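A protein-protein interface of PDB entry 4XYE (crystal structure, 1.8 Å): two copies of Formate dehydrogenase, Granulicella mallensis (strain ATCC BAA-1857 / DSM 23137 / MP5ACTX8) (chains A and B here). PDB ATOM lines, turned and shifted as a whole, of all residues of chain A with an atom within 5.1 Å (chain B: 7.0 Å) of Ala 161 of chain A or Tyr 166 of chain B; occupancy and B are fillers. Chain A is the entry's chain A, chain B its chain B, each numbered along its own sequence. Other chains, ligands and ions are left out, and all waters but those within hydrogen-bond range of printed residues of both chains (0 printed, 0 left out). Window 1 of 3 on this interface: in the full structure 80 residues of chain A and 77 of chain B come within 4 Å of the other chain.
Hydrophobic or aromatic side chains of chain B that line the printed part of chain A: Met 157, Leu 160, Ala 161, Tyr 166, Leu 167 and His 170.
Of the 16 printed residues of chain A, 9 touch a printed residue of chain B.
Hydrophobic or aromatic side chains of chain A within 4 Å of the printed part of chain B: Met 157, Met 158, Leu 160, Ala 161, Tyr 166 and Leu 167.
Among the printed residues, 18 pairs touch across the chains.
Among the printed residues, no Asp or Glu carboxylate lies within 4 Å of a Lys or Arg side-chain nitrogen of the other chain.
The backbone NH (N) of Tyr 166 of chain A lies within hydrogen-bond range of the backbone carbonyl oxygen (O) of Ala 161 of chain A.
The backbone carbonyl oxygen of Ala 161 of chain B sits at hydrogen-bond distance from the backbone NH of Tyr 166 of chain B, 3.0 Å away.
O of Asn 165 of chain B lies within hydrogen-bond range of OG of Ser 169 of chain B (2.8 Å).
OG of Ser 169 of chain B sits close to SG of Cys 183 of chain B, 3.5 Å away.
Met 157 of chain A touches Leu 160 of chain B, and with the chains exchanged Leu 160 of chain A touches Met 157 of chain B.
Ala 161 of chain A touches Tyr 166 of chain B, and with the chains exchanged Tyr 166 of chain A touches Ala 161 of chain B.
Tyr 166 of chain A touches Leu 167 of chain B, and with the chains exchanged Leu 167 of chain A touches Tyr 166 of chain B.
Leu 167 of chain B touches its own counterpart, Leu 167 of chain A.
Of chain B, only Met 157 and Tyr 166 come within 4 Å of Ala 161 of chain A.
Of the printed residues of chain B, Tyr 166 of chain A touches Met 157 (3.5 Å), Ala 161 (3.6 Å) and Leu 167 (3.6 Å).
Of the printed residues of chain A, Met 157 of chain B touches Leu 160 (3.7 Å), Ala 161 (3.7 Å) and Tyr 166 (3.5 Å).
Of the printed residues of chain A, Ala 161 of chain B touches Met 157 (3.8 Å) and Tyr 166 (3.6 Å).
Of the printed residues of chain A, Leu 167 of chain B touches Tyr 166 (3.6 Å) and Leu 167 (3.4 Å).
The nearest residue of chain A that does not touch Tyr 166 of chain B is Met 330 of chain A (4.5 Å).
The backbone carbonyl oxygen (O) of Gly 329 of chain A lies within hydrogen-bond range of the side-chain hydroxyl (OH) of Tyr 166 of chain B, at 2.7 Å.
The backbone carbonyl oxygen (O) of Met 330 of chain A lies within hydrogen-bond range of a ring nitrogen (ND1) of His 170 of chain B (2.7 Å).
The backbone carbonyl oxygen of Leu 160 of chain B lies close to the side-chain sulfur of Met 157 of chain A, 3.8 Å away.
O of Leu 160 of chain A lies close to SD of Met 157 of chain B, 3.7 Å away.
Among the printed residues, merely in contact across the chains: Met 157 of chain A with Ala 161 of chain B, Met 157 of chain A with Tyr 166 of chain B, Met 158 of chain A with Tyr 166 of chain B, Ala 161 of chain A with Met 157 of chain B, Ala 161 of chain A with Tyr 166 of chain B, Tyr 166 of chain A with Met 157 of chain B, Tyr 166 of chain A with Ala 161 of chain B, Tyr 166 of chain A with Leu 167 of chain B, Leu 167 of chain A with Tyr 166 of chain B, Leu 167 of chain A with Leu 167 of chain B, Leu 167 of chain A with His 170 of chain B, Gly 329 of chain A with His 170 of chain B, Thr 331 of chain A with Tyr 166 of chain B and Thr 331 of chain A with Ser 169 of chain B.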
ATOM      1  N   VAL A 156      30.549   9.181 -12.862  1.00  0.00           N
ATOM      2  CA  VAL A 156      30.758   7.752 -13.129  1.00  0.00           C
ATOM      3  C   VAL A 156      30.340   6.884 -11.937  1.00  0.00           C
ATOM      4  O   VAL A 156      29.719   5.826 -12.106  1.00  0.00           O
ATOM      5  CB  VAL A 156      32.206   7.436 -13.554  1.00  0.00           C
ATOM      6  CG1 VAL A 156      32.374   5.917 -13.761  1.00  0.00           C
ATOM      7  CG2 VAL A 156      32.558   8.189 -14.844  1.00  0.00           C
ATOM      8  N   MET A 157      30.659   7.343 -10.732  1.00  0.00           N
ATOM      9  CA  MET A 157      30.192   6.670  -9.518  1.00  0.00           C
ATOM     10  C   MET A 157      28.659   6.536  -9.476  1.00  0.00           C
ATOM     11  O   MET A 157      28.123   5.457  -9.152  1.00  0.00           O
ATOM     12  CB  MET A 157      30.698   7.448  -8.291  1.00  0.00           C
ATOM     13  CG  MET A 157      30.246   6.934  -6.940  1.00  0.00           C
ATOM     14  SD  MET A 157      30.708   8.152  -5.685  1.00  0.00           S
ATOM     15  CE  MET A 157      29.539   9.452  -6.042  1.00  0.00           C
ATOM     16  N   MET A 158      27.951   7.620  -9.806  1.00  0.00           N
ATOM     17  CA  MET A 158      26.481   7.604  -9.802  1.00  0.00           C
ATOM     18  C   MET A 158      25.907   6.704 -10.902  1.00  0.00           C
ATOM     19  O   MET A 158      24.926   5.976 -10.688  1.00  0.00           O
ATOM     20  CB  MET A 158      25.911   9.030  -9.897  1.00  0.00           C
ATOM     21  CG  MET A 158      26.121   9.826  -8.598  1.00  0.00           C
ATOM     22  SD  MET A 158      25.599  11.550  -8.730  1.00  0.00           S
ATOM     23  CE  MET A 158      25.359  11.930  -6.991  1.00  0.00           C
ATOM     24  N   ILE A 159      26.521   6.738 -12.078  1.00  0.00           N
ATOM     25  CA  ILE A 159      26.105   5.816 -13.133  1.00  0.00           C
ATOM     26  C   ILE A 159      26.148   4.374 -12.636  1.00  0.00           C
ATOM     27  O   ILE A 159      25.164   3.631 -12.742  1.00  0.00           O
ATOM     28  CB  ILE A 159      26.977   5.937 -14.393  1.00  0.00           C
ATOM     29  CG1 ILE A 159      26.731   7.278 -15.082  1.00  0.00           C
ATOM     30  CG2 ILE A 159      26.671   4.759 -15.349  1.00  0.00           C
ATOM     31  CD1 ILE A 159      27.724   7.600 -16.206  1.00  0.00           C
ATOM     32  N   LEU A 160      27.284   3.984 -12.069  1.00  0.00           N
ATOM     33  CA  LEU A 160      27.438   2.637 -11.516  1.00  0.00           C
ATOM     34  C   LEU A 160      26.434   2.341 -10.399  1.00  0.00           C
ATOM     35  O   LEU A 160      25.798   1.297 -10.407  1.00  0.00           O
ATOM     36  CB  LEU A 160      28.870   2.408 -11.029  1.00  0.00           C
ATOM     37  CG  LEU A 160      29.935   2.316 -12.133  1.00  0.00           C
ATOM     38  CD1 LEU A 160      31.347   2.481 -11.593  1.00  0.00           C
ATOM     39  CD2 LEU A 160      29.797   0.994 -12.885  1.00  0.00           C
ATOM     40  N   ALA A 161      26.278   3.263  -9.449  1.00  0.00           N
ATOM     41  CA  ALA A 161      25.385   3.008  -8.320  1.00  0.00           C
ATOM     42  C   ALA A 161      23.920   2.806  -8.757  1.00  0.00           C
ATOM     43  O   ALA A 161      23.208   1.958  -8.209  1.00  0.00           O
ATOM     44  CB  ALA A 161      25.503   4.133  -7.294  1.00  0.00           C
ATOM     45  N   LEU A 162      23.467   3.587  -9.734  1.00  0.00           N
ATOM     46  CA  LEU A 162      22.108   3.420 -10.258  1.00  0.00           C
ATOM     47  C   LEU A 162      21.925   2.083 -10.971  1.00  0.00           C
ATOM     48  O   LEU A 162      20.986   1.319 -10.693  1.00  0.00           O
ATOM     49  CB  LEU A 162      21.773   4.548 -11.235  1.00  0.00           C
ATOM     50  CG  LEU A 162      21.529   5.957 -10.698  1.00  0.00           C
ATOM     51  CD1 LEU A 162      21.280   6.921 -11.867  1.00  0.00           C
ATOM     52  CD2 LEU A 162      20.356   5.970  -9.718  1.00  0.00           C
ATOM     53  N   VAL A 163      22.814   1.810 -11.916  1.00  0.00           N
ATOM     54  CA  VAL A 163      22.665   0.620 -12.751  1.00  0.00           C
ATOM     55  C   VAL A 163      22.758  -0.655 -11.913  1.00  0.00           C
ATOM     56  O   VAL A 163      21.989  -1.596 -12.109  1.00  0.00           O
ATOM     57  CB  VAL A 163      23.698   0.625 -13.898  1.00  0.00           C
ATOM     58  CG1 VAL A 163      23.691  -0.688 -14.656  1.00  0.00           C
ATOM     59  CG2 VAL A 163      23.396   1.779 -14.854  1.00  0.00           C
ATOM     60  N   ARG A 164      23.669  -0.663 -10.946  1.00  0.00           N
ATOM     61  CA  ARG A 164      23.901  -1.849 -10.128  1.00  0.00           C
ATOM     62  C   ARG A 164      22.972  -1.957  -8.906  1.00  0.00           C
ATOM     63  O   ARG A 164      23.003  -2.977  -8.196  1.00  0.00           O
ATOM     64  CB  ARG A 164      25.380  -1.922  -9.684  1.00  0.00           C
ATOM     65  CG  ARG A 164      26.412  -1.893 -10.833  1.00  0.00           C
ATOM     66  CD  ARG A 164      27.800  -2.469 -10.411  1.00  0.00           C
ATOM     67  NE  ARG A 164      27.605  -3.840  -9.963  1.00  0.00           N
ATOM     68  CZ  ARG A 164      27.514  -4.885 -10.778  1.00  0.00           C
ATOM     69  NH1 ARG A 164      27.685  -4.734 -12.091  1.00  0.00           N
ATOM     70  NH2 ARG A 164      27.259  -6.091 -10.271  1.00  0.00           N
ATOM     71  N   ASN A 165      22.153  -0.925  -8.671  1.00  0.00           N
ATOM     72  CA  ASN A 165      21.242  -0.875  -7.516  1.00  0.00           C
ATOM     73  C   ASN A 165      21.989  -0.862  -6.179  1.00  0.00           C
ATOM     74  O   ASN A 165      21.608  -1.539  -5.218  1.00  0.00           O
ATOM     75  CB  ASN A 165      20.214  -2.033  -7.548  1.00  0.00           C
ATOM     76  CG  ASN A 165      19.004  -1.769  -6.642  1.00  0.00           C
ATOM     77  OD1 ASN A 165      18.486  -0.648  -6.602  1.00  0.00           O
ATOM     78  ND2 ASN A 165      18.568  -2.792  -5.901  1.00  0.00           N
ATOM     79  N   TYR A 166      23.036  -0.048  -6.105  1.00  0.00           N
ATOM     80  CA  TYR A 166      23.873   0.011  -4.907  1.00  0.00           C
ATOM     81  C   TYR A 166      23.148   0.540  -3.671  1.00  0.00           C
ATOM     82  O   TYR A 166      23.231  -0.055  -2.595  1.00  0.00           O
ATOM     83  CB  TYR A 166      25.083   0.901  -5.195  1.00  0.00           C
ATOM     84  CG  TYR A 166      26.209   0.915  -4.163  1.00  0.00           C
ATOM     85  CD1 TYR A 166      26.286  -0.006  -3.118  1.00  0.00           C
ATOM     86  CD2 TYR A 166      27.211   1.870  -4.256  1.00  0.00           C
ATOM     87  CE1 TYR A 166      27.346   0.034  -2.196  1.00  0.00           C
ATOM     88  CE2 TYR A 166      28.254   1.917  -3.360  1.00  0.00           C
ATOM     89  CZ  TYR A 166      28.327   1.010  -2.334  1.00  0.00           C
ATOM     90  OH  TYR A 166      29.405   1.109  -1.474  1.00  0.00           O
ATOM     91  N   LEU A 167      22.472   1.679  -3.805  1.00  0.00           N
ATOM     92  CA  LEU A 167      21.991   2.383  -2.601  1.00  0.00           C
ATOM     93  C   LEU A 167      20.945   1.641  -1.754  1.00  0.00           C
ATOM     94  O   LEU A 167      21.075   1.586  -0.529  1.00  0.00           O
ATOM     95  CB  LEU A 167      21.542   3.818  -2.916  1.00  0.00           C
ATOM     96  CG  LEU A 167      22.642   4.618  -3.614  1.00  0.00           C
ATOM     97  CD1 LEU A 167      22.148   5.980  -4.038  1.00  0.00           C
ATOM     98  CD2 LEU A 167      23.829   4.760  -2.687  1.00  0.00           C
ATOM     99  N   ALA A 307      20.203  10.265 -10.864  1.00  0.00           N
ATOM    100  CA  ALA A 307      21.125  10.615  -9.789  1.00  0.00           C
ATOM    101  C   ALA A 307      21.884  11.854 -10.199  1.00  0.00           C
ATOM    102  O   ALA A 307      22.150  12.055 -11.377  1.00  0.00           O
ATOM    103  CB  ALA A 307      22.085   9.481  -9.503  1.00  0.00           C
ATOM    104  N   GLY A 329      19.599   8.580  -6.782  1.00  0.00           N
ATOM    105  CA  GLY A 329      20.905   8.466  -6.152  1.00  0.00           C
ATOM    106  C   GLY A 329      21.509   9.813  -5.772  1.00  0.00           C
ATOM    107  O   GLY A 329      22.725   9.990  -5.848  1.00  0.00           O
ATOM    108  N   MET A 330      20.666  10.755  -5.353  1.00  0.00           N
ATOM    109  CA  MET A 330      21.091  12.147  -5.131  1.00  0.00           C
ATOM    110  C   MET A 330      22.108  12.291  -4.005  1.00  0.00           C
ATOM    111  O   MET A 330      22.105  11.517  -3.056  1.00  0.00           O
ATOM    112  CB  MET A 330      19.890  13.038  -4.771  1.00  0.00           C
ATOM    113  CG  MET A 330      18.714  12.989  -5.759  1.00  0.00           C
ATOM    114  SD  MET A 330      19.172  13.513  -7.416  1.00  0.00           S
ATOM    115  CE  MET A 330      19.467  15.268  -7.173  1.00  0.00           C
ATOM    116  N   THR A 331      22.960  13.306  -4.127  1.00  0.00           N
ATOM    117  CA  THR A 331      23.630  13.900  -2.969  1.00  0.00           C
ATOM    118  C   THR A 331      23.385  15.405  -3.014  1.00  0.00           C
ATOM    119  O   THR A 331      23.017  15.950  -4.055  1.00  0.00           O
ATOM    120  CB  THR A 331      25.165  13.682  -3.000  1.00  0.00           C
ATOM    121  OG1 THR A 331      25.708  14.332  -4.154  1.00  0.00           O
ATOM    122  CG2 THR A 331      25.515  12.203  -3.030  1.00  0.00           C
ATOM    123  N   MET B 157      33.016   0.779  -8.305  1.00  0.00           N
ATOM    124  CA  MET B 157      31.934   1.591  -7.759  1.00  0.00           C
ATOM    125  C   MET B 157      32.166   1.839  -6.271  1.00  0.00           C
ATOM    126  O   MET B 157      31.983   2.953  -5.761  1.00  0.00           O
ATOM    127  CB  MET B 157      30.596   0.871  -7.967  1.00  0.00           C
ATOM    128  CG  MET B 157      29.386   1.532  -7.351  1.00  0.00           C
ATOM    129  SD  MET B 157      27.935   0.427  -7.512  1.00  0.00           S
ATOM    130  CE  MET B 157      28.353  -0.816  -6.306  1.00  0.00           C
ATOM    131  N   LEU B 160      35.086   4.314  -5.488  1.00  0.00           N
ATOM    132  CA  LEU B 160      34.650   5.702  -5.652  1.00  0.00           C
ATOM    133  C   LEU B 160      33.742   6.143  -4.508  1.00  0.00           C
ATOM    134  O   LEU B 160      33.927   7.211  -3.925  1.00  0.00           O
ATOM    135  CB  LEU B 160      33.938   5.878  -6.996  1.00  0.00           C
ATOM    136  CG  LEU B 160      34.857   5.760  -8.214  1.00  0.00           C
ATOM    137  CD1 LEU B 160      34.034   5.610  -9.500  1.00  0.00           C
ATOM    138  CD2 LEU B 160      35.757   6.980  -8.312  1.00  0.00           C
ATOM    139  N   ALA B 161      32.759   5.313  -4.181  1.00  0.00           N
ATOM    140  CA  ALA B 161      31.822   5.636  -3.100  1.00  0.00           C
ATOM    141  C   ALA B 161      32.539   5.901  -1.774  1.00  0.00           C
ATOM    142  O   ALA B 161      32.171   6.810  -1.038  1.00  0.00           O
ATOM    143  CB  ALA B 161      30.786   4.511  -2.933  1.00  0.00           C
ATOM    144  N   LEU B 162      33.555   5.101  -1.471  1.00  0.00           N
ATOM    145  CA  LEU B 162      34.312   5.286  -0.229  1.00  0.00           C
ATOM    146  C   LEU B 162      35.123   6.563  -0.231  1.00  0.00           C
ATOM    147  O   LEU B 162      35.056   7.378   0.694  1.00  0.00           O
ATOM    148  CB  LEU B 162      35.265   4.118  -0.010  1.00  0.00           C
ATOM    149  CG  LEU B 162      34.706   2.789   0.496  1.00  0.00           C
ATOM    150  CD1 LEU B 162      35.851   1.791   0.684  1.00  0.00           C
ATOM    151  CD2 LEU B 162      33.919   2.964   1.801  1.00  0.00           C
ATOM    152  N   VAL B 163      35.920   6.741  -1.271  1.00  0.00           N
ATOM    153  CA  VAL B 163      36.829   7.874  -1.324  1.00  0.00           C
ATOM    154  C   VAL B 163      36.050   9.198  -1.358  1.00  0.00           C
ATOM    155  O   VAL B 163      36.440  10.182  -0.725  1.00  0.00           O
ATOM    156  CB  VAL B 163      37.787   7.728  -2.528  1.00  0.00           C
ATOM    157  CG1 VAL B 163      38.620   8.987  -2.725  1.00  0.00           C
ATOM    158  CG2 VAL B 163      38.686   6.507  -2.330  1.00  0.00           C
ATOM    159  N   ARG B 164      34.924   9.194  -2.072  1.00  0.00           N
ATOM    160  CA  ARG B 164      34.138  10.408  -2.292  1.00  0.00           C
ATOM    161  C   ARG B 164      33.103  10.689  -1.190  1.00  0.00           C
ATOM    162  O   ARG B 164      32.521  11.770  -1.156  1.00  0.00           O
ATOM    163  CB  ARG B 164      33.469  10.399  -3.681  1.00  0.00           C
ATOM    164  CG  ARG B 164      34.451  10.261  -4.857  1.00  0.00           C
ATOM    165  CD  ARG B 164      33.837  10.770  -6.183  1.00  0.00           C
ATOM    166  NE  ARG B 164      33.458  12.169  -6.022  1.00  0.00           N
ATOM    167  CZ  ARG B 164      34.305  13.187  -6.134  1.00  0.00           C
ATOM    168  NH1 ARG B 164      35.566  12.960  -6.464  1.00  0.00           N
ATOM    169  NH2 ARG B 164      33.886  14.430  -5.929  1.00  0.00           N
ATOM    170  N   ASN B 165      32.883   9.714  -0.305  1.00  0.00           N
ATOM    171  CA  ASN B 165      31.928   9.848   0.806  1.00  0.00           C
ATOM    172  C   ASN B 165      30.473   9.896   0.327  1.00  0.00           C
ATOM    173  O   ASN B 165      29.669  10.684   0.820  1.00  0.00           O
ATOM    174  CB  ASN B 165      32.235  11.067   1.705  1.00  0.00           C
ATOM    175  CG  ASN B 165      31.587  10.950   3.078  1.00  0.00           C
ATOM    176  OD1 ASN B 165      31.567   9.863   3.652  1.00  0.00           O
ATOM    177  ND2 ASN B 165      31.040  12.062   3.605  1.00  0.00           N
ATOM    178  N   TYR B 166      30.146   9.025  -0.627  1.00  0.00           N
ATOM    179  CA  TYR B 166      28.845   9.027  -1.287  1.00  0.00           C
ATOM    180  C   TYR B 166      27.710   8.659  -0.331  1.00  0.00           C
ATOM    181  O   TYR B 166      26.678   9.333  -0.283  1.00  0.00           O
ATOM    182  CB  TYR B 166      28.880   8.027  -2.446  1.00  0.00           C
ATOM    183  CG  TYR B 166      27.675   7.998  -3.373  1.00  0.00           C
ATOM    184  CD1 TYR B 166      26.690   8.979  -3.333  1.00  0.00           C
ATOM    185  CD2 TYR B 166      27.532   6.971  -4.302  1.00  0.00           C
ATOM    186  CE1 TYR B 166      25.586   8.938  -4.199  1.00  0.00           C
ATOM    187  CE2 TYR B 166      26.454   6.929  -5.168  1.00  0.00           C
ATOM    188  CZ  TYR B 166      25.487   7.915  -5.114  1.00  0.00           C
ATOM    189  OH  TYR B 166      24.420   7.857  -5.980  1.00  0.00           O
ATOM    190  N   LEU B 167      27.883   7.561   0.398  1.00  0.00           N
ATOM    191  CA  LEU B 167      26.761   6.975   1.120  1.00  0.00           C
ATOM    192  C   LEU B 167      26.187   7.864   2.239  1.00  0.00           C
ATOM    193  O   LEU B 167      24.970   8.021   2.332  1.00  0.00           O
ATOM    194  CB  LEU B 167      27.105   5.557   1.626  1.00  0.00           C
ATOM    195  CG  LEU B 167      27.561   4.614   0.504  1.00  0.00           C
ATOM    196  CD1 LEU B 167      27.958   3.247   1.027  1.00  0.00           C
ATOM    197  CD2 LEU B 167      26.461   4.444  -0.496  1.00  0.00           C
ATOM    198  N   PRO B 168      27.053   8.443   3.100  1.00  0.00           N
ATOM    199  CA  PRO B 168      26.491   9.326   4.127  1.00  0.00           C
ATOM    200  C   PRO B 168      25.883  10.580   3.498  1.00  0.00           C
ATOM    201  O   PRO B 168      24.957  11.175   4.049  1.00  0.00           O
ATOM    202  CB  PRO B 168      27.717   9.708   4.967  1.00  0.00           C
ATOM    203  CG  PRO B 168      28.665   8.590   4.779  1.00  0.00           C
ATOM    204  CD  PRO B 168      28.484   8.186   3.331  1.00  0.00           C
ATOM    205  N   SER B 169      26.415  10.984   2.348  1.00  0.00           N
ATOM    206  CA  SER B 169      25.926  12.186   1.688  1.00  0.00           C
ATOM    207  C   SER B 169      24.541  11.958   1.053  1.00  0.00           C
ATOM    208  O   SER B 169      23.684  12.847   1.051  1.00  0.00           O
ATOM    209  CB  SER B 169      26.940  12.669   0.665  1.00  0.00           C
ATOM    210  OG  SER B 169      28.156  13.023   1.304  1.00  0.00           O
ATOM    211  N   HIS B 170      24.329  10.764   0.520  1.00  0.00           N
ATOM    212  CA  HIS B 170      23.009  10.396   0.008  1.00  0.00           C
ATOM    213  C   HIS B 170      21.968  10.402   1.136  1.00  0.00           C
ATOM    214  O   HIS B 170      20.832  10.805   0.940  1.00  0.00           O
ATOM    215  CB  HIS B 170      23.062   9.023  -0.659  1.00  0.00           C
ATOM    216  CG  HIS B 170      21.735   8.550  -1.165  1.00  0.00           C
ATOM    217  ND1 HIS B 170      21.031   9.221  -2.142  1.00  0.00           N
ATOM    218  CD2 HIS B 170      20.981   7.478  -0.822  1.00  0.00           C
ATOM    219  CE1 HIS B 170      19.902   8.577  -2.386  1.00  0.00           C
ATOM    220  NE2 HIS B 170      19.845   7.520  -1.596  1.00  0.00           N
ATOM    221  N   LYS B 171      22.375   9.947   2.316  1.00  0.00           N
ATOM    222  CA  LYS B 171      21.476   9.875   3.465  1.00  0.00           C
ATOM    223  C   LYS B 171      21.050  11.286   3.860  1.00  0.00           C
ATOM    224  O   LYS B 171      19.879  11.531   4.159  1.00  0.00           O
ATOM    225  CB  LYS B 171      22.180   9.169   4.626  1.00  0.00           C
ATOM    226  CG  LYS B 171      21.329   8.906   5.858  1.00  0.00           C
ATOM    227  CD  LYS B 171      22.162   8.113   6.869  1.00  0.00           C
ATOM    228  CE  LYS B 171      21.312   7.519   7.978  1.00  0.00           C
ATOM    229  NZ  LYS B 171      21.535   8.230   9.263  1.00  0.00           N
ATOM    230  N   ILE B 172      22.005  12.214   3.847  1.00  0.00           N
ATOM    231  CA  ILE B 172      21.694  13.623   4.095  1.00  0.00           C
ATOM    232  C   ILE B 172      20.667  14.181   3.102  1.00  0.00           C
ATOM    233  O   ILE B 172      19.745  14.902   3.493  1.00  0.00           O
ATOM    234  CB  ILE B 172      22.963  14.481   4.092  1.00  0.00           C
ATOM    235  CG1 ILE B 172      23.805  14.138   5.325  1.00  0.00           C
ATOM    236  CG2 ILE B 172      22.612  15.978   4.037  1.00  0.00           C
ATOM    237  CD1 ILE B 172      25.197  14.744   5.307  1.00  0.00           C
ATOM    238  N   CYS B 183      29.224  16.797   4.342  1.00  0.00           N
ATOM    239  CA  CYS B 183      29.427  15.874   3.224  1.00  0.00           C
ATOM    240  C   CYS B 183      30.893  15.790   2.787  1.00  0.00           C
ATOM    241  O   CYS B 183      31.397  14.710   2.490  1.00  0.00           O
ATOM    242  CB  CYS B 183      28.596  16.296   2.003  1.00  0.00           C
ATOM    243  SG  CYS B 183      26.797  16.122   2.164  1.00  0.00           S
ATOM    244  N   SER B 187      35.559  13.919   2.021  1.00  0.00           N
ATOM    245  CA  SER B 187      35.435  13.605   0.595  1.00  0.00           C
ATOM    246  C   SER B 187      36.703  13.952  -0.186  1.00  0.00           C
ATOM    247  O   SER B 187      37.184  15.092  -0.144  1.00  0.00           O
ATOM    248  CB  SER B 187      34.215  14.316  -0.015  1.00  0.00           C
ATOM    249  OG  SER B 187      34.040  13.990  -1.389  1.00  0.00           O
